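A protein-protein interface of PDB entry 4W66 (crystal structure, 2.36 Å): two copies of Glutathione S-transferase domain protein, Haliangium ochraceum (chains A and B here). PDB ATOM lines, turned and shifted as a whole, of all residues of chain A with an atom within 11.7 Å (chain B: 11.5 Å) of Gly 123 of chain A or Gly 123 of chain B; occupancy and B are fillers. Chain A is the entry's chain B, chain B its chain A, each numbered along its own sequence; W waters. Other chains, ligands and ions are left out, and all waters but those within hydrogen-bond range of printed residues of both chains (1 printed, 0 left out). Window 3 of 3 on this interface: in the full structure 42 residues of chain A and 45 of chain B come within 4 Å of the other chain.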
ATOM      1  N   TRP A 116     -12.614 -11.692   0.345  1.00  0.00           N
ATOM      2  CA  TRP A 116     -12.069 -11.158   1.575  1.00  0.00           C
ATOM      3  C   TRP A 116     -11.612 -12.253   2.542  1.00  0.00           C
ATOM      4  O   TRP A 116     -11.159 -11.942   3.634  1.00  0.00           O
ATOM      5  CB  TRP A 116     -13.122 -10.298   2.272  1.00  0.00           C
ATOM      6  CG  TRP A 116     -13.355  -8.984   1.636  1.00  0.00           C
ATOM      7  CD1 TRP A 116     -14.400  -8.642   0.846  1.00  0.00           C
ATOM      8  CD2 TRP A 116     -12.538  -7.809   1.759  1.00  0.00           C
ATOM      9  NE1 TRP A 116     -14.288  -7.333   0.459  1.00  0.00           N
ATOM     10  CE2 TRP A 116     -13.150  -6.799   1.001  1.00  0.00           C
ATOM     11  CE3 TRP A 116     -11.362  -7.513   2.448  1.00  0.00           C
ATOM     12  CZ2 TRP A 116     -12.619  -5.510   0.896  1.00  0.00           C
ATOM     13  CZ3 TRP A 116     -10.831  -6.230   2.344  1.00  0.00           C
ATOM     14  CH2 TRP A 116     -11.458  -5.247   1.569  1.00  0.00           C
ATOM     15  N   LEU A 117     -11.717 -13.519   2.153  1.00  0.00           N
ATOM     16  CA  LEU A 117     -11.637 -14.606   3.114  1.00  0.00           C
ATOM     17  C   LEU A 117     -10.349 -14.639   3.943  1.00  0.00           C
ATOM     18  O   LEU A 117     -10.428 -14.753   5.170  1.00  0.00           O
ATOM     19  CB  LEU A 117     -11.864 -15.971   2.454  1.00  0.00           C
ATOM     20  CG  LEU A 117     -12.408 -17.007   3.458  1.00  0.00           C
ATOM     21  CD1 LEU A 117     -13.898 -16.762   3.710  1.00  0.00           C
ATOM     22  CD2 LEU A 117     -12.180 -18.438   3.001  1.00  0.00           C
ATOM     23  N   ASP A 118      -9.185 -14.525   3.303  1.00  0.00           N
ATOM     24  CA  ASP A 118      -7.936 -14.589   4.050  1.00  0.00           C
ATOM     25  C   ASP A 118      -7.515 -13.248   4.660  1.00  0.00           C
ATOM     26  O   ASP A 118      -6.531 -13.182   5.400  1.00  0.00           O
ATOM     27  CB  ASP A 118      -6.809 -15.237   3.233  1.00  0.00           C
ATOM     28  CG  ASP A 118      -6.167 -14.294   2.222  1.00  0.00           C
ATOM     29  OD1 ASP A 118      -6.743 -13.221   1.900  1.00  0.00           O
ATOM     30  OD2 ASP A 118      -5.062 -14.655   1.735  1.00  0.00           O
ATOM     31  N   LEU A 119      -8.235 -12.174   4.364  1.00  0.00           N
ATOM     32  CA  LEU A 119      -8.030 -10.949   5.129  1.00  0.00           C
ATOM     33  C   LEU A 119      -8.917 -10.917   6.388  1.00  0.00           C
ATOM     34  O   LEU A 119      -8.576 -10.278   7.387  1.00  0.00           O
ATOM     35  CB  LEU A 119      -8.260  -9.720   4.260  1.00  0.00           C
ATOM     36  CG  LEU A 119      -7.190  -9.474   3.208  1.00  0.00           C
ATOM     37  CD1 LEU A 119      -7.491  -8.179   2.471  1.00  0.00           C
ATOM     38  CD2 LEU A 119      -5.810  -9.403   3.837  1.00  0.00           C
ATOM     39  N   PHE A 120     -10.035 -11.628   6.347  1.00  0.00           N
ATOM     40  CA  PHE A 120     -10.976 -11.646   7.471  1.00  0.00           C
ATOM     41  C   PHE A 120     -10.820 -12.853   8.363  1.00  0.00           C
ATOM     42  O   PHE A 120     -11.158 -12.792   9.525  1.00  0.00           O
ATOM     43  CB  PHE A 120     -12.421 -11.495   6.970  1.00  0.00           C
ATOM     44  CG  PHE A 120     -12.867 -10.078   6.975  1.00  0.00           C
ATOM     45  CD1 PHE A 120     -12.575  -9.251   5.906  1.00  0.00           C
ATOM     46  CD2 PHE A 120     -13.484  -9.541   8.102  1.00  0.00           C
ATOM     47  CE1 PHE A 120     -12.941  -7.918   5.923  1.00  0.00           C
ATOM     48  CE2 PHE A 120     -13.858  -8.212   8.138  1.00  0.00           C
ATOM     49  CZ  PHE A 120     -13.583  -7.395   7.042  1.00  0.00           C
ATOM     50  N   ASN A 121     -10.277 -13.928   7.810  1.00  0.00           N
ATOM     51  CA  ASN A 121      -9.996 -15.136   8.547  1.00  0.00           C
ATOM     52  C   ASN A 121      -8.505 -15.473   8.481  1.00  0.00           C
ATOM     53  O   ASN A 121      -8.121 -16.545   7.990  1.00  0.00           O
ATOM     54  CB  ASN A 121     -10.835 -16.271   7.974  1.00  0.00           C
ATOM     55  CG  ASN A 121     -12.316 -15.993   8.085  1.00  0.00           C
ATOM     56  OD1 ASN A 121     -12.952 -16.395   9.049  1.00  0.00           O
ATOM     57  ND2 ASN A 121     -12.860 -15.256   7.127  1.00  0.00           N
ATOM     58  N   PRO A 122      -7.652 -14.564   8.986  1.00  0.00           N
ATOM     59  CA  PRO A 122      -6.212 -14.745   8.843  1.00  0.00           C
ATOM     60  C   PRO A 122      -5.793 -16.141   9.240  1.00  0.00           C
ATOM     61  O   PRO A 122      -6.221 -16.631  10.290  1.00  0.00           O
ATOM     62  CB  PRO A 122      -5.612 -13.706   9.804  1.00  0.00           C
ATOM     63  CG  PRO A 122      -6.754 -13.159  10.592  1.00  0.00           C
ATOM     64  CD  PRO A 122      -7.978 -13.354   9.754  1.00  0.00           C
ATOM     65  N   GLY A 123      -4.990 -16.779   8.390  1.00  0.00           N
ATOM     66  CA  GLY A 123      -4.492 -18.117   8.647  1.00  0.00           C
ATOM     67  C   GLY A 123      -5.326 -19.220   8.039  1.00  0.00           C
ATOM     68  O   GLY A 123      -4.951 -20.383   8.095  1.00  0.00           O
ATOM     69  N   VAL A 124      -6.469 -18.876   7.456  1.00  0.00           N
ATOM     70  CA  VAL A 124      -7.319 -19.896   6.840  1.00  0.00           C
ATOM     71  C   VAL A 124      -6.582 -20.693   5.761  1.00  0.00           C
ATOM     72  O   VAL A 124      -5.812 -20.120   4.981  1.00  0.00           O
ATOM     73  CB  VAL A 124      -8.614 -19.309   6.237  1.00  0.00           C
ATOM     74  CG1 VAL A 124      -8.328 -18.227   5.202  1.00  0.00           C
ATOM     75  CG2 VAL A 124      -9.458 -20.423   5.628  1.00  0.00           C
ATOM     76  N   ASP A 125      -6.828 -22.006   5.744  1.00  0.00           N
ATOM     77  CA  ASP A 125      -6.475 -22.859   4.619  1.00  0.00           C
ATOM     78  C   ASP A 125      -7.566 -22.791   3.526  1.00  0.00           C
ATOM     79  O   ASP A 125      -8.631 -23.416   3.645  1.00  0.00           O
ATOM     80  CB  ASP A 125      -6.260 -24.305   5.084  1.00  0.00           C
ATOM     81  CG  ASP A 125      -5.658 -25.185   3.994  1.00  0.00           C
ATOM     82  OD1 ASP A 125      -6.366 -25.486   3.009  1.00  0.00           O
ATOM     83  OD2 ASP A 125      -4.477 -25.579   4.119  1.00  0.00           O
ATOM     84  N   LEU A 126      -7.273 -22.052   2.454  1.00  0.00           N
ATOM     85  CA  LEU A 126      -8.226 -21.828   1.350  1.00  0.00           C
ATOM     86  C   LEU A 126      -8.665 -23.088   0.607  1.00  0.00           C
ATOM     87  O   LEU A 126      -9.803 -23.181   0.160  1.00  0.00           O
ATOM     88  CB  LEU A 126      -7.639 -20.844   0.337  1.00  0.00           C
ATOM     89  CG  LEU A 126      -7.317 -19.432   0.833  1.00  0.00           C
ATOM     90  CD1 LEU A 126      -6.832 -18.595  -0.333  1.00  0.00           C
ATOM     91  CD2 LEU A 126      -8.518 -18.763   1.495  1.00  0.00           C
ATOM     92  N   ALA A 127      -7.764 -24.050   0.478  1.00  0.00           N
ATOM     93  CA  ALA A 127      -8.033 -25.266  -0.276  1.00  0.00           C
ATOM     94  C   ALA A 127      -9.141 -26.119   0.338  1.00  0.00           C
ATOM     95  O   ALA A 127      -9.835 -26.838  -0.373  1.00  0.00           O
ATOM     96  CB  ALA A 127      -6.756 -26.083  -0.421  1.00  0.00           C
ATOM     97  N   ALA A 128      -9.304 -26.058   1.654  1.00  0.00           N
ATOM     98  CA  ALA A 128     -10.400 -26.781   2.308  1.00  0.00           C
ATOM     99  C   ALA A 128     -11.642 -25.893   2.448  1.00  0.00           C
ATOM    100  O   ALA A 128     -12.767 -26.321   2.165  1.00  0.00           O
ATOM    101  CB  ALA A 128      -9.952 -27.305   3.664  1.00  0.00           C
ATOM    102  N   ALA A 129     -11.418 -24.649   2.858  1.00  0.00           N
ATOM    103  CA  ALA A 129     -12.500 -23.700   3.148  1.00  0.00           C
ATOM    104  C   ALA A 129     -13.372 -23.366   1.936  1.00  0.00           C
ATOM    105  O   ALA A 129     -14.600 -23.456   1.994  1.00  0.00           O
ATOM    106  CB  ALA A 129     -11.911 -22.416   3.731  1.00  0.00           C
ATOM    107  N   VAL A 130     -12.721 -22.989   0.841  1.00  0.00           N
ATOM    108  CA  VAL A 130     -13.411 -22.474  -0.344  1.00  0.00           C
ATOM    109  C   VAL A 130     -14.326 -23.487  -1.032  1.00  0.00           C
ATOM    110  O   VAL A 130     -15.483 -23.181  -1.293  1.00  0.00           O
ATOM    111  CB  VAL A 130     -12.417 -21.892  -1.371  1.00  0.00           C
ATOM    112  CG1 VAL A 130     -13.109 -21.610  -2.697  1.00  0.00           C
ATOM    113  CG2 VAL A 130     -11.767 -20.627  -0.829  1.00  0.00           C
ATOM    114  N   LEU A 132     -15.992 -25.797   0.092  1.00  0.00           N
ATOM    115  CA  LEU A 132     -17.200 -26.006   0.895  1.00  0.00           C
ATOM    116  C   LEU A 132     -18.164 -24.814   0.809  1.00  0.00           C
ATOM    117  O   LEU A 132     -19.350 -24.994   0.566  1.00  0.00           O
ATOM    118  CB  LEU A 132     -16.834 -26.298   2.355  1.00  0.00           C
ATOM    119  CG  LEU A 132     -17.995 -26.583   3.323  1.00  0.00           C
ATOM    120  CD1 LEU A 132     -19.037 -27.525   2.724  1.00  0.00           C
ATOM    121  CD2 LEU A 132     -17.455 -27.143   4.634  1.00  0.00           C
ATOM    122  N   GLN A 133     -17.637 -23.607   0.995  1.00  0.00           N
ATOM    123  CA  GLN A 133     -18.436 -22.377   0.929  1.00  0.00           C
ATOM    124  C   GLN A 133     -18.878 -22.059  -0.489  1.00  0.00           C
ATOM    125  O   GLN A 133     -19.979 -21.565  -0.706  1.00  0.00           O
ATOM    126  CB  GLN A 133     -17.651 -21.200   1.499  1.00  0.00           C
ATOM    127  CG  GLN A 133     -17.395 -21.334   2.988  1.00  0.00           C
ATOM    128  CD  GLN A 133     -16.572 -20.192   3.553  1.00  0.00           C
ATOM    129  OE1 GLN A 133     -16.831 -19.027   3.260  1.00  0.00           O
ATOM    130  NE2 GLN A 133     -15.578 -20.523   4.376  1.00  0.00           N
ATOM    131  N   MET A 225      -5.830 -11.808  -5.662  1.00  0.00           N
ATOM    132  CA  MET A 225      -6.683 -12.734  -4.913  1.00  0.00           C
ATOM    133  C   MET A 225      -7.416 -13.684  -5.824  1.00  0.00           C
ATOM    134  O   MET A 225      -7.504 -14.874  -5.537  1.00  0.00           O
ATOM    135  CB  MET A 225      -7.665 -11.938  -4.047  1.00  0.00           C
ATOM    136  CG  MET A 225      -8.438 -12.825  -3.079  1.00  0.00           C
ATOM    137  SD  MET A 225      -7.245 -13.769  -1.816  1.00  0.00           S
ATOM    138  CE  MET A 225      -7.913 -15.583  -2.190  1.00  0.00           C
ATOM    139  N   ARG A 228      -5.301 -16.561  -7.053  1.00  0.00           N
ATOM    140  CA  ARG A 228      -5.157 -17.593  -6.024  1.00  0.00           C
ATOM    141  C   ARG A 228      -6.379 -18.500  -5.985  1.00  0.00           C
ATOM    142  O   ARG A 228      -6.242 -19.719  -5.912  1.00  0.00           O
ATOM    143  CB  ARG A 228      -4.893 -16.975  -4.641  1.00  0.00           C
ATOM    144  CG  ARG A 228      -3.442 -16.570  -4.419  1.00  0.00           C
ATOM    145  CD  ARG A 228      -3.251 -15.659  -3.208  1.00  0.00           C
ATOM    146  NE  ARG A 228      -3.761 -16.231  -1.954  1.00  0.00           N
ATOM    147  CZ  ARG A 228      -3.182 -17.217  -1.262  1.00  0.00           C
ATOM    148  NH1 ARG A 228      -2.055 -17.794  -1.678  1.00  0.00           N
ATOM    149  NH2 ARG A 228      -3.738 -17.643  -0.138  1.00  0.00           N
ATOM    150  N   TRP B 116     -19.617 -20.989  13.748  1.00  0.00           N
ATOM    151  CA  TRP B 116     -19.212 -21.998  12.769  1.00  0.00           C
ATOM    152  C   TRP B 116     -17.823 -21.759  12.184  1.00  0.00           C
ATOM    153  O   TRP B 116     -17.437 -22.446  11.252  1.00  0.00           O
ATOM    154  CB  TRP B 116     -20.219 -22.039  11.613  1.00  0.00           C
ATOM    155  CG  TRP B 116     -21.493 -22.737  11.917  1.00  0.00           C
ATOM    156  CD1 TRP B 116     -22.717 -22.165  12.118  1.00  0.00           C
ATOM    157  CD2 TRP B 116     -21.686 -24.147  12.040  1.00  0.00           C
ATOM    158  NE1 TRP B 116     -23.659 -23.133  12.362  1.00  0.00           N
ATOM    159  CE2 TRP B 116     -23.052 -24.359  12.318  1.00  0.00           C
ATOM    160  CE3 TRP B 116     -20.841 -25.252  11.939  1.00  0.00           C
ATOM    161  CZ2 TRP B 116     -23.589 -25.634  12.497  1.00  0.00           C
ATOM    162  CZ3 TRP B 116     -21.377 -26.522  12.127  1.00  0.00           C
ATOM    163  CH2 TRP B 116     -22.736 -26.699  12.400  1.00  0.00           C
ATOM    164  N   LEU B 117     -17.065 -20.805  12.715  1.00  0.00           N
ATOM    165  CA  LEU B 117     -15.865 -20.335  12.014  1.00  0.00           C
ATOM    166  C   LEU B 117     -14.815 -21.422  11.791  1.00  0.00           C
ATOM    167  O   LEU B 117     -14.203 -21.474  10.724  1.00  0.00           O
ATOM    168  CB  LEU B 117     -15.225 -19.137  12.722  1.00  0.00           C
ATOM    169  CG  LEU B 117     -14.492 -18.179  11.772  1.00  0.00           C
ATOM    170  CD1 LEU B 117     -15.470 -17.486  10.817  1.00  0.00           C
ATOM    171  CD2 LEU B 117     -13.676 -17.145  12.541  1.00  0.00           C
ATOM    172  N   ASP B 118     -14.603 -22.275  12.788  1.00  0.00           N
ATOM    173  CA  ASP B 118     -13.653 -23.391  12.666  1.00  0.00           C
ATOM    174  C   ASP B 118     -13.975 -24.290  11.500  1.00  0.00           C
ATOM    175  O   ASP B 118     -13.121 -24.550  10.651  1.00  0.00           O
ATOM    176  CB  ASP B 118     -13.658 -24.272  13.923  1.00  0.00           C
ATOM    177  CG  ASP B 118     -12.675 -23.811  14.960  1.00  0.00           C
ATOM    178  OD1 ASP B 118     -11.594 -23.309  14.572  1.00  0.00           O
ATOM    179  OD2 ASP B 118     -12.979 -23.966  16.166  1.00  0.00           O
ATOM    180  N   LEU B 119     -15.213 -24.763  11.480  1.00  0.00           N
ATOM    181  CA  LEU B 119     -15.633 -25.794  10.548  1.00  0.00           C
ATOM    182  C   LEU B 119     -15.842 -25.281   9.126  1.00  0.00           C
ATOM    183  O   LEU B 119     -15.878 -26.073   8.182  1.00  0.00           O
ATOM    184  CB  LEU B 119     -16.916 -26.451  11.051  1.00  0.00           C
ATOM    185  CG  LEU B 119     -16.782 -27.120  12.425  1.00  0.00           C
ATOM    186  CD1 LEU B 119     -18.157 -27.435  13.008  1.00  0.00           C
ATOM    187  CD2 LEU B 119     -15.907 -28.373  12.354  1.00  0.00           C
ATOM    188  N   PHE B 120     -16.002 -23.967   8.979  1.00  0.00           N
ATOM    189  CA  PHE B 120     -16.182 -23.345   7.665  1.00  0.00           C
ATOM    190  C   PHE B 120     -14.880 -22.736   7.144  1.00  0.00           C
ATOM    191  O   PHE B 120     -14.704 -22.625   5.935  1.00  0.00           O
ATOM    192  CB  PHE B 120     -17.304 -22.291   7.717  1.00  0.00           C
ATOM    193  CG  PHE B 120     -18.679 -22.837   7.405  1.00  0.00           C
ATOM    194  CD1 PHE B 120     -19.022 -24.162   7.695  1.00  0.00           C
ATOM    195  CD2 PHE B 120     -19.646 -22.015   6.839  1.00  0.00           C
ATOM    196  CE1 PHE B 120     -20.289 -24.655   7.407  1.00  0.00           C
ATOM    197  CE2 PHE B 120     -20.914 -22.501   6.551  1.00  0.00           C
ATOM    198  CZ  PHE B 120     -21.235 -23.823   6.836  1.00  0.00           C
ATOM    199  N   ASN B 121     -13.985 -22.346   8.054  1.00  0.00           N
ATOM    200  CA  ASN B 121     -12.654 -21.843   7.708  1.00  0.00           C
ATOM    201  C   ASN B 121     -11.513 -22.600   8.437  1.00  0.00           C
ATOM    202  O   ASN B 121     -10.908 -22.055   9.375  1.00  0.00           O
ATOM    203  CB  ASN B 121     -12.564 -20.351   8.042  1.00  0.00           C
ATOM    204  CG  ASN B 121     -13.651 -19.537   7.382  1.00  0.00           C
ATOM    205  OD1 ASN B 121     -13.513 -19.119   6.242  1.00  0.00           O
ATOM    206  ND2 ASN B 121     -14.737 -19.302   8.100  1.00  0.00           N
ATOM    207  N   PRO B 122     -11.205 -23.847   8.008  1.00  0.00           N
ATOM    208  CA  PRO B 122     -10.143 -24.643   8.652  1.00  0.00           C
ATOM    209  C   PRO B 122      -8.783 -23.935   8.698  1.00  0.00           C
ATOM    210  O   PRO B 122      -8.406 -23.255   7.738  1.00  0.00           O
ATOM    211  CB  PRO B 122     -10.049 -25.896   7.769  1.00  0.00           C
ATOM    212  CG  PRO B 122     -11.366 -25.994   7.091  1.00  0.00           C
ATOM    213  CD  PRO B 122     -11.836 -24.581   6.898  1.00  0.00           C
ATOM    214  N   GLY B 123      -8.068 -24.090   9.811  1.00  0.00           N
ATOM    215  CA  GLY B 123      -6.748 -23.473   9.993  1.00  0.00           C
ATOM    216  C   GLY B 123      -6.781 -21.995  10.354  1.00  0.00           C
ATOM    217  O   GLY B 123      -5.736 -21.360  10.467  1.00  0.00           O
ATOM    218  N   VAL B 124      -7.975 -21.438  10.553  1.00  0.00           N
ATOM    219  CA  VAL B 124      -8.087 -20.031  10.907  1.00  0.00           C
ATOM    220  C   VAL B 124      -7.583 -19.800  12.336  1.00  0.00           C
ATOM    221  O   VAL B 124      -7.809 -20.617  13.229  1.00  0.00           O
ATOM    222  CB  VAL B 124      -9.532 -19.501  10.757  1.00  0.00           C
ATOM    223  CG1 VAL B 124     -10.475 -20.162  11.760  1.00  0.00           C
ATOM    224  CG2 VAL B 124      -9.563 -17.985  10.916  1.00  0.00           C
ATOM    225  N   ASP B 125      -6.891 -18.680  12.524  1.00  0.00           N
ATOM    226  CA  ASP B 125      -6.433 -18.234  13.824  1.00  0.00           C
ATOM    227  C   ASP B 125      -7.555 -17.421  14.488  1.00  0.00           C
ATOM    228  O   ASP B 125      -7.762 -16.245  14.168  1.00  0.00           O
ATOM    229  CB  ASP B 125      -5.170 -17.381  13.637  1.00  0.00           C
ATOM    230  CG  ASP B 125      -4.387 -17.188  14.920  1.00  0.00           C
ATOM    231  OD1 ASP B 125      -4.955 -16.695  15.912  1.00  0.00           O
ATOM    232  OD2 ASP B 125      -3.184 -17.519  14.932  1.00  0.00           O
ATOM    233  N   LEU B 126      -8.278 -18.057  15.408  1.00  0.00           N
ATOM    234  CA  LEU B 126      -9.378 -17.416  16.111  1.00  0.00           C
ATOM    235  C   LEU B 126      -8.955 -16.104  16.757  1.00  0.00           C
ATOM    236  O   LEU B 126      -9.661 -15.102  16.641  1.00  0.00           O
ATOM    237  CB  LEU B 126      -9.964 -18.351  17.179  1.00  0.00           C
ATOM    238  CG  LEU B 126     -10.750 -19.574  16.664  1.00  0.00           C
ATOM    239  CD1 LEU B 126     -11.344 -20.399  17.808  1.00  0.00           C
ATOM    240  CD2 LEU B 126     -11.850 -19.149  15.699  1.00  0.00           C
ATOM    241  N   ALA B 127      -7.798 -16.103  17.410  1.00  0.00           N
ATOM    242  CA  ALA B 127      -7.310 -14.912  18.099  1.00  0.00           C
ATOM    243  C   ALA B 127      -7.137 -13.694  17.190  1.00  0.00           C
ATOM    244  O   ALA B 127      -7.255 -12.560  17.652  1.00  0.00           O
ATOM    245  CB  ALA B 127      -6.003 -15.213  18.817  1.00  0.00           C
ATOM    246  N   ALA B 128      -6.827 -13.920  15.917  1.00  0.00           N
ATOM    247  CA  ALA B 128      -6.702 -12.821  14.944  1.00  0.00           C
ATOM    248  C   ALA B 128      -8.050 -12.480  14.292  1.00  0.00           C
ATOM    249  O   ALA B 128      -8.422 -11.300  14.188  1.00  0.00           O
ATOM    250  CB  ALA B 128      -5.674 -13.173  13.880  1.00  0.00           C
ATOM    251  N   ALA B 129      -8.782 -13.521  13.888  1.00  0.00           N
ATOM    252  CA  ALA B 129     -10.008 -13.368  13.091  1.00  0.00           C
ATOM    253  C   ALA B 129     -11.211 -12.815  13.865  1.00  0.00           C
ATOM    254  O   ALA B 129     -12.002 -12.028  13.331  1.00  0.00           O
ATOM    255  CB  ALA B 129     -10.374 -14.708  12.469  1.00  0.00           C
ATOM    256  N   VAL B 130     -11.364 -13.246  15.113  1.00  0.00           N
ATOM    257  CA  VAL B 130     -12.554 -12.912  15.879  1.00  0.00           C
ATOM    258  C   VAL B 130     -12.603 -11.413  16.206  1.00  0.00           C
ATOM    259  O   VAL B 130     -13.598 -10.760  15.902  1.00  0.00           O
ATOM    260  CB  VAL B 130     -12.713 -13.820  17.123  1.00  0.00           C
ATOM    261  CG1 VAL B 130     -13.850 -13.345  18.020  1.00  0.00           C
ATOM    262  CG2 VAL B 130     -12.977 -15.257  16.691  1.00  0.00           C
ATOM    263  N   LEU B 132     -11.600  -8.851  14.735  1.00  0.00           N
ATOM    264  CA  LEU B 132     -11.993  -8.096  13.540  1.00  0.00           C
ATOM    265  C   LEU B 132     -13.480  -8.199  13.248  1.00  0.00           C
ATOM    266  O   LEU B 132     -14.161  -7.197  13.110  1.00  0.00           O
ATOM    267  CB  LEU B 132     -11.251  -8.609  12.303  1.00  0.00           C
ATOM    268  CG  LEU B 132      -9.757  -8.314  12.244  1.00  0.00           C
ATOM    269  CD1 LEU B 132      -9.157  -8.963  10.994  1.00  0.00           C
ATOM    270  CD2 LEU B 132      -9.483  -6.803  12.303  1.00  0.00           C
ATOM    271  N   GLN B 133     -13.959  -9.427  13.114  1.00  0.00           N
ATOM    272  CA  GLN B 133     -15.326  -9.671  12.697  1.00  0.00           C
ATOM    273  C   GLN B 133     -16.288  -9.179  13.783  1.00  0.00           C
ATOM    274  O   GLN B 133     -17.259  -8.466  13.514  1.00  0.00           O
ATOM    275  CB  GLN B 133     -15.499 -11.154  12.339  1.00  0.00           C
ATOM    276  CG  GLN B 133     -14.738 -11.499  11.056  1.00  0.00           C
ATOM    277  CD  GLN B 133     -14.724 -12.976  10.709  1.00  0.00           C
ATOM    278  OE1 GLN B 133     -15.763 -13.585  10.528  1.00  0.00           O
ATOM    279  NE2 GLN B 133     -13.529 -13.552  10.591  1.00  0.00           N
ATOM    280  N   MET B 225     -17.465 -24.333  21.482  1.00  0.00           N
ATOM    281  CA  MET B 225     -17.091 -23.148  20.723  1.00  0.00           C
ATOM    282  C   MET B 225     -17.207 -21.889  21.523  1.00  0.00           C
ATOM    283  O   MET B 225     -16.340 -21.031  21.433  1.00  0.00           O
ATOM    284  CB  MET B 225     -17.907 -23.016  19.448  1.00  0.00           C
ATOM    285  CG  MET B 225     -17.087 -23.515  18.263  1.00  0.00           C
ATOM    286  SD  MET B 225     -15.376 -22.521  18.088  1.00  0.00           S
ATOM    287  CE  MET B 225     -15.876 -20.832  17.210  1.00  0.00           C
ATOM    288  N   ARG B 228     -14.231 -21.259  23.900  1.00  0.00           N
ATOM    289  CA  ARG B 228     -13.105 -20.791  23.081  1.00  0.00           C
ATOM    290  C   ARG B 228     -13.261 -19.325  22.698  1.00  0.00           C
ATOM    291  O   ARG B 228     -12.323 -18.543  22.822  1.00  0.00           O
ATOM    292  CB  ARG B 228     -12.908 -21.646  21.828  1.00  0.00           C
ATOM    293  CG  ARG B 228     -11.644 -22.488  21.886  1.00  0.00           C
ATOM    294  CD  ARG B 228     -11.455 -23.324  20.636  1.00  0.00           C
ATOM    295  NE  ARG B 228     -12.603 -24.204  20.431  1.00  0.00           N
ATOM    296  CZ  ARG B 228     -12.821 -24.932  19.337  1.00  0.00           C
ATOM    297  NH1 ARG B 228     -11.960 -24.913  18.322  1.00  0.00           N
ATOM    298  NH2 ARG B 228     -13.915 -25.686  19.257  1.00  0.00           N
HETATM  299  O   HOH W   1      -3.075 -20.556  10.687  1.00  0.00           O
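The backbone carbonyl oxygen (O) of Phe 120 of chain B sits at hydrogen-bond distance from the side-chain amide nitrogen (NE2) of Gln 133 of chain A (2.8 Å).
NE2 of Gln 133 of chain A is in hydrogen-bond range of OD1 of Asn 121 of chain B (3.1 Å).
N of Asp 125 of chain A is in hydrogen-bond range of O of Pro 122 of chain B (2.8 Å).
The backbone carbonyl oxygen (O) of Gly 123 of chain B lies close to the backbone carbonyl oxygen (O) of Gly 123 of chain A, 2.7 Å away.
The backbone carbonyl oxygen of Pro 122 of chain A sits at hydrogen-bond distance from the backbone NH of Asp 125 of chain B, at 3.1 Å.
The backbone carbonyl oxygen (O) of Phe 120 of chain A is in hydrogen-bond range of the side-chain amide nitrogen (NE2) of Gln 133 of chain B.
The side-chain amide oxygen (OD1) of Asn 121 of chain A lies within hydrogen-bond range of the side-chain amide nitrogen (NE2) of Gln 133 of chain B, 3.3 Å away.
O of Leu 117 of chain B lies close to ND2 of Asn 121 of chain B, at 3.4 Å.
OD1 of Asp 125 of chain B is in hydrogen-bond range of N of Ala 128 of chain B.
The side-chain amide nitrogen (NE2) of Gln 133 of chain B sits at hydrogen-bond distance from the backbone carbonyl oxygen (O) of Ala 129 of chain B.
The backbone carbonyl oxygen (O) of Leu 117 of chain A is in hydrogen-bond range of the side-chain amide nitrogen (ND2) of Asn 121 of chain A, 3.2 Å away.
Asn 121 of chain B touches Leu 117 of chain A.
Leu 117 of chain B touches Asn 121 of chain A (CD1 to OD1, 3.3 Å).
Asn 121 of chain A touches Val 124 of chain B.
Asn 121 of chain A touches Ala 129 of chain B.
Pro 122 of chain A touches Ala 128 of chain B.
Val 124 of chain A touches Asn 121 of chain B (CG2 to CB, 3.9 Å).
Val 124 of chain A touches Gly 123 of chain B.
N of Val 124 of chain A touches CA of Val 124 of chain B, 3.98 Å away.
Ala 128 of chain A touches Pro 122 of chain B.
Pro 122 of chain B touches Ala 129 of chain A.
Gly 123 of chain A touches just one residue of chain B: Gly 123.
Gly 123 of chain B touches just these residues of chain A: Gly 123 (2.7 Å) and Val 124 (3.97 Å).
Of chain B, only Val 124, Asp 125, Ala 128 and Ala 129 come within 4 Å of Pro 122 of chain A.
Pro 122 of chain B touches four residues of chain A.
Of chain A, only Pro 122 comes within 4 Å of Asp 125 of chain B.
Printed residues of chain B within 4 Å of Leu 119 of chain A: Leu 132 (3.9 Å).
Of the printed residues of chain A, Ala 128 of chain B touches Pro 122.
Asp 118 of chain A touches none of the printed residues of chain B.
The nearest printed residue of chain A that does not touch Leu 132 of chain B is Phe 120 of chain A (4.6 Å).
Hydrophobic or aromatic side chains of chain B that line the printed part of chain A: Leu 117, Pro 122, Val 124, Ala 128, Ala 129 and Leu 132.
Of the 19 printed residues of chain A, 11 touch a printed residue of chain B.
Printed residues of chain A that touch a printed residue of chain B: Leu 117, Leu 119, Phe 120, Asn 121, Pro 122, Gly 123, Val 124, Asp 125, Ala 128, Ala 129 and Gln 133.
Leu 117 of chain A touches Asn 121 of chain B, and with the chains exchanged Asn 121 of chain A touches Leu 117 of chain B.
Pro 122 of chain A touches Val 124 of chain B, and with the chains exchanged Val 124 of chain A touches Pro 122 of chain B.
Pro 122 of chain A touches Ala 128 of chain B, and with the chains exchanged Ala 128 of chain A touches Pro 122 of chain B.
Val 124 of chain A touches Gly 123 of chain B, but with the chains exchanged Gly 123 of chain A does not touch Val 124 of chain B (4.04 Å).
Water W1 lies within hydrogen-bond range of the backbone carbonyl oxygen (O) of Gly 123 of chain B (2.8 Å) and the backbone carbonyl oxygen (O) of Gly 123 of chain A (3.2 Å).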
